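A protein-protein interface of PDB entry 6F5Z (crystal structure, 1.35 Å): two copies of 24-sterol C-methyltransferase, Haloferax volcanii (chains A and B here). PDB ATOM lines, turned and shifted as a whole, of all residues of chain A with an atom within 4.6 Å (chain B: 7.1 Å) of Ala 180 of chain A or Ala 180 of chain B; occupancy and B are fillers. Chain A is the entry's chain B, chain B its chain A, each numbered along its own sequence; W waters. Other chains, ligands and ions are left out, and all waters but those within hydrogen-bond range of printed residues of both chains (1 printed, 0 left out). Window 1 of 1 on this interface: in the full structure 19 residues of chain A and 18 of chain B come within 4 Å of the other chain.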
ATOM      1  N   PRO A  35      -4.013   2.205 -34.588  1.00  0.00           N
ATOM      2  CA  PRO A  35      -5.211   2.520 -35.398  1.00  0.00           C
ATOM      3  C   PRO A  35      -5.133   3.898 -36.047  1.00  0.00           C
ATOM      4  O   PRO A  35      -6.015   4.744 -35.891  1.00  0.00           O
ATOM      5  CB  PRO A  35      -6.316   2.479 -34.335  1.00  0.00           C
ATOM      6  CG  PRO A  35      -5.655   3.000 -33.144  1.00  0.00           C
ATOM      7  CD  PRO A  35      -4.258   2.428 -33.144  1.00  0.00           C
ATOM      8  N   THR A 135      -4.569   7.108 -28.789  1.00  0.00           N
ATOM      9  CA  THR A 135      -3.924   5.985 -28.121  1.00  0.00           C
ATOM     10  C   THR A 135      -2.491   6.243 -27.771  1.00  0.00           C
ATOM     11  O   THR A 135      -1.842   7.113 -28.365  1.00  0.00           O
ATOM     12  CB  THR A 135      -3.956   4.678 -28.974  1.00  0.00           C
ATOM     13  OG1 THR A 135      -3.052   4.795 -30.090  1.00  0.00           O
ATOM     14  CG2 THR A 135      -5.380   4.307 -29.431  1.00  0.00           C
ATOM     15  N   TYR A 137       0.831   3.838 -27.337  1.00  0.00           N
ATOM     16  CA  TYR A 137       1.437   2.524 -27.546  1.00  0.00           C
ATOM     17  C   TYR A 137       2.785   2.562 -26.813  1.00  0.00           C
ATOM     18  O   TYR A 137       3.696   3.281 -27.255  1.00  0.00           O
ATOM     19  CB  TYR A 137       1.611   2.252 -29.055  1.00  0.00           C
ATOM     20  CG  TYR A 137       0.395   1.583 -29.652  1.00  0.00           C
ATOM     21  CD1 TYR A 137      -0.823   2.250 -29.740  1.00  0.00           C
ATOM     22  CD2 TYR A 137       0.461   0.278 -30.127  1.00  0.00           C
ATOM     23  CE1 TYR A 137      -1.972   1.604 -30.203  1.00  0.00           C
ATOM     24  CE2 TYR A 137      -0.673  -0.376 -30.614  1.00  0.00           C
ATOM     25  CZ  TYR A 137      -1.891   0.283 -30.634  1.00  0.00           C
ATOM     26  OH  TYR A 137      -3.002  -0.394 -31.081  1.00  0.00           O
ATOM     27  N   HIS A 178      -7.585   4.318 -20.460  1.00  0.00           N
ATOM     28  CA  HIS A 178      -8.225   2.995 -20.426  1.00  0.00           C
ATOM     29  C   HIS A 178      -7.255   2.011 -21.061  1.00  0.00           C
ATOM     30  O   HIS A 178      -6.694   2.316 -22.105  1.00  0.00           O
ATOM     31  CB  HIS A 178      -9.474   2.984 -21.307  1.00  0.00           C
ATOM     32  CG  HIS A 178     -10.526   3.951 -20.876  1.00  0.00           C
ATOM     33  ND1 HIS A 178     -11.082   4.854 -21.771  1.00  0.00           N
ATOM     34  CD2 HIS A 178     -11.095   4.113 -19.663  1.00  0.00           C
ATOM     35  CE1 HIS A 178     -11.992   5.523 -21.077  1.00  0.00           C
ATOM     36  NE2 HIS A 178     -12.031   5.118 -19.804  1.00  0.00           N
ATOM     37  N   VAL A 179      -7.076   0.831 -20.467  1.00  0.00           N
ATOM     38  CA  VAL A 179      -6.158  -0.162 -21.068  1.00  0.00           C
ATOM     39  C   VAL A 179      -6.946  -0.962 -22.098  1.00  0.00           C
ATOM     40  O   VAL A 179      -7.931  -1.635 -21.748  1.00  0.00           O
ATOM     41  CB  VAL A 179      -5.526  -1.069 -19.991  1.00  0.00           C
ATOM     42  CG1 VAL A 179      -4.644  -2.148 -20.609  1.00  0.00           C
ATOM     43  CG2 VAL A 179      -4.726  -0.251 -18.983  1.00  0.00           C
ATOM     44  N   ALA A 180      -6.483  -0.915 -23.353  1.00  0.00           N
ATOM     45  CA  ALA A 180      -7.190  -1.617 -24.435  1.00  0.00           C
ATOM     46  C   ALA A 180      -6.601  -2.958 -24.806  1.00  0.00           C
ATOM     47  O   ALA A 180      -7.306  -3.794 -25.383  1.00  0.00           O
ATOM     48  CB  ALA A 180      -7.241  -0.740 -25.680  1.00  0.00           C
ATOM     49  N   GLU A 181      -5.303  -3.138 -24.528  1.00  0.00           N
ATOM     50  CA  GLU A 181      -4.605  -4.324 -24.947  1.00  0.00           C
ATOM     51  C   GLU A 181      -3.313  -4.389 -24.180  1.00  0.00           C
ATOM     52  O   GLU A 181      -2.728  -3.342 -23.860  1.00  0.00           O
ATOM     53  CB  GLU A 181      -4.268  -4.168 -26.456  1.00  0.00           C
ATOM     54  CG  GLU A 181      -3.772  -5.437 -27.095  1.00  0.00           C
ATOM     55  CD  GLU A 181      -2.318  -5.432 -27.521  1.00  0.00           C
ATOM     56  OE1 GLU A 181      -1.452  -5.788 -26.692  1.00  0.00           O
ATOM     57  OE2 GLU A 181      -2.047  -5.126 -28.702  1.00  0.00           O
ATOM     58  N   VAL A 222      -1.335  -0.817 -24.400  1.00  0.00           N
ATOM     59  CA  VAL A 222      -2.041   0.202 -25.197  1.00  0.00           C
ATOM     60  C   VAL A 222      -3.083   0.889 -24.324  1.00  0.00           C
ATOM     61  O   VAL A 222      -3.901   0.187 -23.712  1.00  0.00           O
ATOM     62  CB  VAL A 222      -2.731  -0.450 -26.402  1.00  0.00           C
ATOM     63  CG1 VAL A 222      -3.554   0.563 -27.216  1.00  0.00           C
ATOM     64  CG2 VAL A 222      -1.681  -1.116 -27.309  1.00  0.00           C
ATOM     65  N   VAL A 224      -5.987   4.247 -23.980  1.00  0.00           N
ATOM     66  CA  VAL A 224      -6.841   5.137 -24.748  1.00  0.00           C
ATOM     67  C   VAL A 224      -7.210   6.317 -23.845  1.00  0.00           C
ATOM     68  O   VAL A 224      -7.584   6.113 -22.679  1.00  0.00           O
ATOM     69  CB  VAL A 224      -8.111   4.414 -25.246  1.00  0.00           C
ATOM     70  CG1 VAL A 224      -9.073   5.412 -25.893  1.00  0.00           C
ATOM     71  CG2 VAL A 224      -7.744   3.336 -26.253  1.00  0.00           C
ATOM     72  N   ARG B  33      -4.170 -11.065 -25.628  1.00  0.00           N
ATOM     73  CA  ARG B  33      -3.866  -9.642 -25.479  1.00  0.00           C
ATOM     74  C   ARG B  33      -5.004  -8.854 -24.865  1.00  0.00           C
ATOM     75  O   ARG B  33      -4.836  -7.668 -24.577  1.00  0.00           O
ATOM     76  CB  ARG B  33      -3.397  -9.025 -26.808  1.00  0.00           C
ATOM     77  CG  ARG B  33      -4.542  -8.845 -27.801  1.00  0.00           C
ATOM     78  CD  ARG B  33      -4.057  -8.399 -29.187  1.00  0.00           C
ATOM     79  NE  ARG B  33      -3.358  -9.484 -29.874  1.00  0.00           N
ATOM     80  CZ  ARG B  33      -2.879  -9.402 -31.114  1.00  0.00           C
ATOM     81  NH1 ARG B  33      -3.038  -8.281 -31.828  1.00  0.00           N
ATOM     82  NH2 ARG B  33      -2.214 -10.427 -31.646  1.00  0.00           N
ATOM     83  N   MET B  34      -6.184  -9.485 -24.659  1.00  0.00           N
ATOM     84  CA  MET B  34      -7.306  -8.733 -24.084  1.00  0.00           C
ATOM     85  C   MET B  34      -6.983  -8.334 -22.661  1.00  0.00           C
ATOM     86  O   MET B  34      -6.440  -9.138 -21.909  1.00  0.00           O
ATOM     87  CB  MET B  34      -8.588  -9.601 -24.001  1.00  0.00           C
ATOM     88  CG  MET B  34      -9.207  -9.866 -25.305  1.00  0.00           C
ATOM     89  SD  MET B  34     -10.861 -10.676 -25.116  1.00  0.00           S
ATOM     90  CE  MET B  34     -11.872  -9.368 -24.535  1.00  0.00           C
ATOM     91  N   PRO B  35      -7.357  -7.120 -22.274  1.00  0.00           N
ATOM     92  CA  PRO B  35      -6.999  -6.618 -20.933  1.00  0.00           C
ATOM     93  C   PRO B  35      -8.020  -7.009 -19.871  1.00  0.00           C
ATOM     94  O   PRO B  35      -8.495  -6.172 -19.084  1.00  0.00           O
ATOM     95  CB  PRO B  35      -6.949  -5.116 -21.176  1.00  0.00           C
ATOM     96  CG  PRO B  35      -8.073  -4.878 -22.153  1.00  0.00           C
ATOM     97  CD  PRO B  35      -8.007  -6.065 -23.090  1.00  0.00           C
ATOM     98  N   HIS B 106     -16.134  -6.547 -20.891  1.00  0.00           N
ATOM     99  CA  HIS B 106     -15.564  -6.750 -22.241  1.00  0.00           C
ATOM    100  C   HIS B 106     -16.508  -7.596 -23.062  1.00  0.00           C
ATOM    101  O   HIS B 106     -17.193  -8.478 -22.515  1.00  0.00           O
ATOM    102  CB  HIS B 106     -14.207  -7.469 -22.165  1.00  0.00           C
ATOM    103  CG  HIS B 106     -13.208  -6.682 -21.371  1.00  0.00           C
ATOM    104  ND1 HIS B 106     -12.909  -6.970 -20.025  1.00  0.00           N
ATOM    105  CD2 HIS B 106     -12.530  -5.577 -21.738  1.00  0.00           C
ATOM    106  CE1 HIS B 106     -12.062  -6.020 -19.641  1.00  0.00           C
ATOM    107  NE2 HIS B 106     -11.834  -5.140 -20.620  1.00  0.00           N
ATOM    108  N   GLY B 133     -14.762   2.385 -20.873  1.00  0.00           N
ATOM    109  CA  GLY B 133     -13.408   1.866 -20.824  1.00  0.00           C
ATOM    110  C   GLY B 133     -13.328   0.379 -21.131  1.00  0.00           C
ATOM    111  O   GLY B 133     -12.222  -0.172 -21.280  1.00  0.00           O
ATOM    112  N   THR B 135     -13.779  -3.118 -23.423  1.00  0.00           N
ATOM    113  CA  THR B 135     -13.390  -3.316 -24.820  1.00  0.00           C
ATOM    114  C   THR B 135     -14.285  -4.249 -25.576  1.00  0.00           C
ATOM    115  O   THR B 135     -14.906  -5.128 -24.991  1.00  0.00           O
ATOM    116  CB  THR B 135     -11.929  -3.871 -24.952  1.00  0.00           C
ATOM    117  OG1 THR B 135     -11.869  -5.228 -24.516  1.00  0.00           O
ATOM    118  CG2 THR B 135     -10.888  -3.022 -24.233  1.00  0.00           C
ATOM    119  N   TYR B 137     -13.546  -6.831 -28.664  1.00  0.00           N
ATOM    120  CA  TYR B 137     -12.562  -7.519 -29.520  1.00  0.00           C
ATOM    121  C   TYR B 137     -13.368  -8.177 -30.615  1.00  0.00           C
ATOM    122  O   TYR B 137     -14.079  -9.157 -30.347  1.00  0.00           O
ATOM    123  CB  TYR B 137     -11.753  -8.556 -28.718  1.00  0.00           C
ATOM    124  CG  TYR B 137     -10.507  -7.948 -28.105  1.00  0.00           C
ATOM    125  CD1 TYR B 137     -10.595  -6.863 -27.229  1.00  0.00           C
ATOM    126  CD2 TYR B 137      -9.240  -8.421 -28.436  1.00  0.00           C
ATOM    127  CE1 TYR B 137      -9.445  -6.240 -26.735  1.00  0.00           C
ATOM    128  CE2 TYR B 137      -8.089  -7.818 -27.933  1.00  0.00           C
ATOM    129  CZ  TYR B 137      -8.194  -6.711 -27.115  1.00  0.00           C
ATOM    130  OH  TYR B 137      -7.020  -6.121 -26.664  1.00  0.00           O
ATOM    131  N   PHE B 172     -16.946   1.473 -36.198  1.00  0.00           N
ATOM    132  CA  PHE B 172     -16.769   1.538 -34.743  1.00  0.00           C
ATOM    133  C   PHE B 172     -16.955   2.978 -34.239  1.00  0.00           C
ATOM    134  O   PHE B 172     -17.694   3.214 -33.271  1.00  0.00           O
ATOM    135  CB  PHE B 172     -15.363   1.039 -34.357  1.00  0.00           C
ATOM    136  CG  PHE B 172     -15.255  -0.461 -34.204  1.00  0.00           C
ATOM    137  CD1 PHE B 172     -15.887  -1.322 -35.102  1.00  0.00           C
ATOM    138  CD2 PHE B 172     -14.519  -1.014 -33.156  1.00  0.00           C
ATOM    139  CE1 PHE B 172     -15.796  -2.713 -34.946  1.00  0.00           C
ATOM    140  CE2 PHE B 172     -14.438  -2.405 -33.003  1.00  0.00           C
ATOM    141  CZ  PHE B 172     -15.043  -3.236 -33.912  1.00  0.00           C
ATOM    142  N   LEU B 177     -17.685   3.907 -30.465  1.00  0.00           N
ATOM    143  CA  LEU B 177     -16.537   3.239 -29.880  1.00  0.00           C
ATOM    144  C   LEU B 177     -15.250   3.931 -30.344  1.00  0.00           C
ATOM    145  O   LEU B 177     -15.149   4.306 -31.514  1.00  0.00           O
ATOM    146  CB  LEU B 177     -16.484   1.780 -30.384  1.00  0.00           C
ATOM    147  CG  LEU B 177     -17.619   0.865 -29.892  1.00  0.00           C
ATOM    148  CD1 LEU B 177     -17.661  -0.468 -30.701  1.00  0.00           C
ATOM    149  CD2 LEU B 177     -17.498   0.613 -28.354  1.00  0.00           C
ATOM    150  N   HIS B 178     -14.282   4.092 -29.448  1.00  0.00           N
ATOM    151  CA  HIS B 178     -12.942   4.542 -29.852  1.00  0.00           C
ATOM    152  C   HIS B 178     -12.215   3.322 -30.456  1.00  0.00           C
ATOM    153  O   HIS B 178     -12.409   2.217 -29.965  1.00  0.00           O
ATOM    154  CB  HIS B 178     -12.134   4.983 -28.641  1.00  0.00           C
ATOM    155  CG  HIS B 178     -12.754   6.108 -27.854  1.00  0.00           C
ATOM    156  ND1 HIS B 178     -13.150   7.269 -28.464  1.00  0.00           N
ATOM    157  CD2 HIS B 178     -12.998   6.192 -26.527  1.00  0.00           C
ATOM    158  CE1 HIS B 178     -13.596   8.058 -27.490  1.00  0.00           C
ATOM    159  NE2 HIS B 178     -13.536   7.444 -26.306  1.00  0.00           N
ATOM    160  N   VAL B 179     -11.390   3.512 -31.486  1.00  0.00           N
ATOM    161  CA  VAL B 179     -10.656   2.371 -32.062  1.00  0.00           C
ATOM    162  C   VAL B 179      -9.254   2.390 -31.434  1.00  0.00           C
ATOM    163  O   VAL B 179      -8.507   3.377 -31.592  1.00  0.00           O
ATOM    164  CB  VAL B 179     -10.598   2.456 -33.603  1.00  0.00           C
ATOM    165  CG1 VAL B 179      -9.850   1.264 -34.168  1.00  0.00           C
ATOM    166  CG2 VAL B 179     -12.018   2.488 -34.188  1.00  0.00           C
ATOM    167  N   ALA B 180      -8.909   1.312 -30.712  1.00  0.00           N
ATOM    168  CA  ALA B 180      -7.645   1.252 -30.020  1.00  0.00           C
ATOM    169  C   ALA B 180      -6.555   0.511 -30.745  1.00  0.00           C
ATOM    170  O   ALA B 180      -5.391   0.738 -30.460  1.00  0.00           O
ATOM    171  CB  ALA B 180      -7.838   0.593 -28.658  1.00  0.00           C
ATOM    172  N   GLU B 181      -6.948  -0.393 -31.641  1.00  0.00           N
ATOM    173  CA  GLU B 181      -6.027  -1.308 -32.293  1.00  0.00           C
ATOM    174  C   GLU B 181      -6.701  -1.916 -33.473  1.00  0.00           C
ATOM    175  O   GLU B 181      -7.892  -2.196 -33.408  1.00  0.00           O
ATOM    176  CB  GLU B 181      -5.637  -2.467 -31.321  1.00  0.00           C
ATOM    177  CG  GLU B 181      -4.823  -3.545 -32.028  1.00  0.00           C
ATOM    178  CD  GLU B 181      -4.130  -4.500 -31.097  1.00  0.00           C
ATOM    179  OE1 GLU B 181      -3.580  -4.024 -30.081  1.00  0.00           O
ATOM    180  OE2 GLU B 181      -4.089  -5.709 -31.418  1.00  0.00           O
ATOM    181  N   GLN B 182      -5.924  -2.176 -34.540  1.00  0.00           N
ATOM    182  CA  GLN B 182      -6.454  -3.000 -35.601  1.00  0.00           C
ATOM    183  C   GLN B 182      -5.275  -3.804 -36.086  1.00  0.00           C
ATOM    184  O   GLN B 182      -4.247  -3.215 -36.437  1.00  0.00           O
ATOM    185  CB  GLN B 182      -7.114  -2.202 -36.701  1.00  0.00           C
ATOM    186  CG  GLN B 182      -7.845  -3.128 -37.682  1.00  0.00           C
ATOM    187  CD  GLN B 182      -8.610  -2.300 -38.688  1.00  0.00           C
ATOM    188  OE1 GLN B 182      -7.987  -1.489 -39.405  1.00  0.00           O
ATOM    189  NE2 GLN B 182      -9.933  -2.471 -38.769  1.00  0.00           N
ATOM    190  N   THR B 221     -10.276  -5.951 -34.779  1.00  0.00           N
ATOM    191  CA  THR B 221     -10.435  -4.513 -34.540  1.00  0.00           C
ATOM    192  C   THR B 221     -10.868  -4.398 -33.062  1.00  0.00           C
ATOM    193  O   THR B 221     -11.787  -5.118 -32.630  1.00  0.00           O
ATOM    194  CB  THR B 221     -11.499  -3.881 -35.446  1.00  0.00           C
ATOM    195  OG1 THR B 221     -11.226  -4.244 -36.802  1.00  0.00           O
ATOM    196  CG2 THR B 221     -11.508  -2.364 -35.333  1.00  0.00           C
ATOM    197  N   VAL B 222     -10.190  -3.540 -32.282  1.00  0.00           N
ATOM    198  CA  VAL B 222     -10.473  -3.393 -30.850  1.00  0.00           C
ATOM    199  C   VAL B 222     -11.135  -2.056 -30.621  1.00  0.00           C
ATOM    200  O   VAL B 222     -10.564  -1.026 -30.979  1.00  0.00           O
ATOM    201  CB  VAL B 222      -9.178  -3.496 -30.004  1.00  0.00           C
ATOM    202  CG1 VAL B 222      -9.473  -3.244 -28.522  1.00  0.00           C
ATOM    203  CG2 VAL B 222      -8.496  -4.857 -30.207  1.00  0.00           C
ATOM    204  N   GLY B 223     -12.340  -2.089 -30.064  1.00  0.00           N
ATOM    205  CA  GLY B 223     -13.064  -0.876 -29.729  1.00  0.00           C
ATOM    206  C   GLY B 223     -13.097  -0.669 -28.226  1.00  0.00           C
ATOM    207  O   GLY B 223     -12.957  -1.625 -27.442  1.00  0.00           O
ATOM    208  N   VAL B 224     -13.181   0.604 -27.800  1.00  0.00           N
ATOM    209  CA  VAL B 224     -13.250   0.941 -26.380  1.00  0.00           C
ATOM    210  C   VAL B 224     -14.507   1.787 -26.198  1.00  0.00           C
ATOM    211  O   VAL B 224     -14.699   2.774 -26.916  1.00  0.00           O
ATOM    212  CB  VAL B 224     -11.969   1.656 -25.869  1.00  0.00           C
ATOM    213  CG1 VAL B 224     -12.125   2.168 -24.442  1.00  0.00           C
ATOM    214  CG2 VAL B 224     -10.760   0.707 -25.955  1.00  0.00           C
HETATM  215  O   HOH W   1     -10.265  -1.839 -20.422  1.00  0.00           O
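O of Arg 33 of chain B lies within hydrogen-bond range of OH of Tyr 137 of chain B, 3.4 Å away. OE2 of Glu 181 of chain B lies within salt-bridge range of NH1 of Arg 33 of chain B (2.8 Å). The backbone carbonyl oxygen (O) of His 178 of chain B lies within hydrogen-bond range of the backbone NH (N) of Val 224 of chain B. The backbone carbonyl oxygen (O) of Val 222 of chain B lies within hydrogen-bond range of the backbone NH (N) of Ala 180 of chain B (2.9 Å). The backbone NH (N) of Val 222 of chain B is in hydrogen-bond range of the backbone carbonyl oxygen (O) of Glu 181 of chain B (2.9 Å). N of Val 222 of chain A lies within hydrogen-bond range of O of Glu 181 of chain A, 2.9 Å away.
Pro 35 of chain A touches Glu 181 of chain B, but with the chains exchanged Glu 181 of chain A does not touch Pro 35 of chain B (4.04 Å). Thr 135 of chain A touches Ala 180 of chain B, and with the chains exchanged Ala 180 of chain A touches Thr 135 of chain B. Tyr 137 of chain A touches Ala 180 of chain B, and with the chains exchanged Ala 180 of chain A touches Tyr 137 of chain B. Ala 180 of chain A touches Val 224 of chain B, and with the chains exchanged Val 224 of chain A touches Ala 180 of chain B. Of the 21 pairs that touch across the chains among the printed residues, 16 have their exchanged pair printed and touching as well.
Of the printed residues of chain B, Pro 35 of chain A touches Val 179, Ala 180 and Glu 181. Ala 180 of chain A touches just these residues of chain B: Pro 35, Thr 135, Tyr 137, Ala 180, Val 222 and Val 224. Printed residues of chain A within 4 Å of Pro 35 of chain B: Val 179 (3.3 Å) and Ala 180 (3.3 Å). Printed residues of chain A within 4 Å of Val 179 of chain B: Pro 35 (3.3 Å) and Thr 135 (3.9 Å). Ala 180 of chain B touches just these residues of chain A: Pro 35, Thr 135, Tyr 137, Ala 180, Val 222 and Val 224. Printed residues of chain A within 4 Å of Val 222 of chain B: Ala 180 (3.9 Å). The nearest printed residue of chain A that does not touch Ala 180 of chain B is Glu 181 of chain A (6.1 Å). The nearest printed residue of chain A that does not touch Gly 133 of chain B is Val 179 of chain A (4.6 Å).
Glu 181 of chain B touches Pro 35 of chain A. CG2 of Thr 135 of chain A touches O of Ala 180 of chain B, at 3.7 Å. Tyr 137 of chain A touches Glu 181 of chain B. CD2 of His 178 of chain A touches CA of Gly 133 of chain B, 3.4 Å away. ND1 of His 178 of chain A touches CG1 of Val 224 of chain B (3.9 Å). Ala 180 of chain A touches Ala 180 of chain B. Val 222 of chain B touches Ala 180 of chain A. CA of Glu 181 of chain A touches O of Arg 33 of chain B, at 3.4 Å. Glu 181 of chain A touches Tyr 137 of chain B. Val 224 of chain A touches Ala 180 of chain B (CG2 to CB, 3.6 Å).
OH of Tyr 137 of chain B lies within hydrogen-bond range of O of Ala 180 of chain A. OH of Tyr 137 of chain A is in hydrogen-bond range of O of Ala 180 of chain B, at 2.7 Å. OE2 of Glu 181 of chain A lies close to OE1 of Glu 181 of chain B (2.3 Å).
Of the 9 printed residues of chain A, 9 touch a printed residue of chain B. Printed residues of chain A that touch a printed residue of chain B: Pro 35, Thr 135, Tyr 137, His 178, Val 179, Ala 180, Glu 181, Val 222 and Val 224. Hydrophobic or aromatic side chains of chain A within 4 Å of the printed part of chain B: Pro 35, Tyr 137, His 178, Val 179, Ala 180, Val 222 and Val 224. Of the 18 printed residues of chain B, 10 touch a printed residue of chain A. Printed residues of chain B that touch a printed residue of chain A: Arg 33, Pro 35, Gly 133, Thr 135, Tyr 137, Val 179, Ala 180, Glu 181, Val 222 and Val 224. Hydrophobic or aromatic side chains of chain B within 4 Å of the printed part of chain A: Pro 35, Tyr 137, Val 179, Ala 180, Val 222 and Val 224. Among the printed residues, 21 pairs touch across the chains. Among the printed residues, no Asp or Glu carboxylate lies within 4 Å of a Lys or Arg side-chain nitrogen of the other chain.
Water W1 lies within hydrogen-bond range of the backbone carbonyl oxygen (O) of Val 179 of chain A and the backbone carbonyl oxygen (O) of Gly 133 of chain B.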
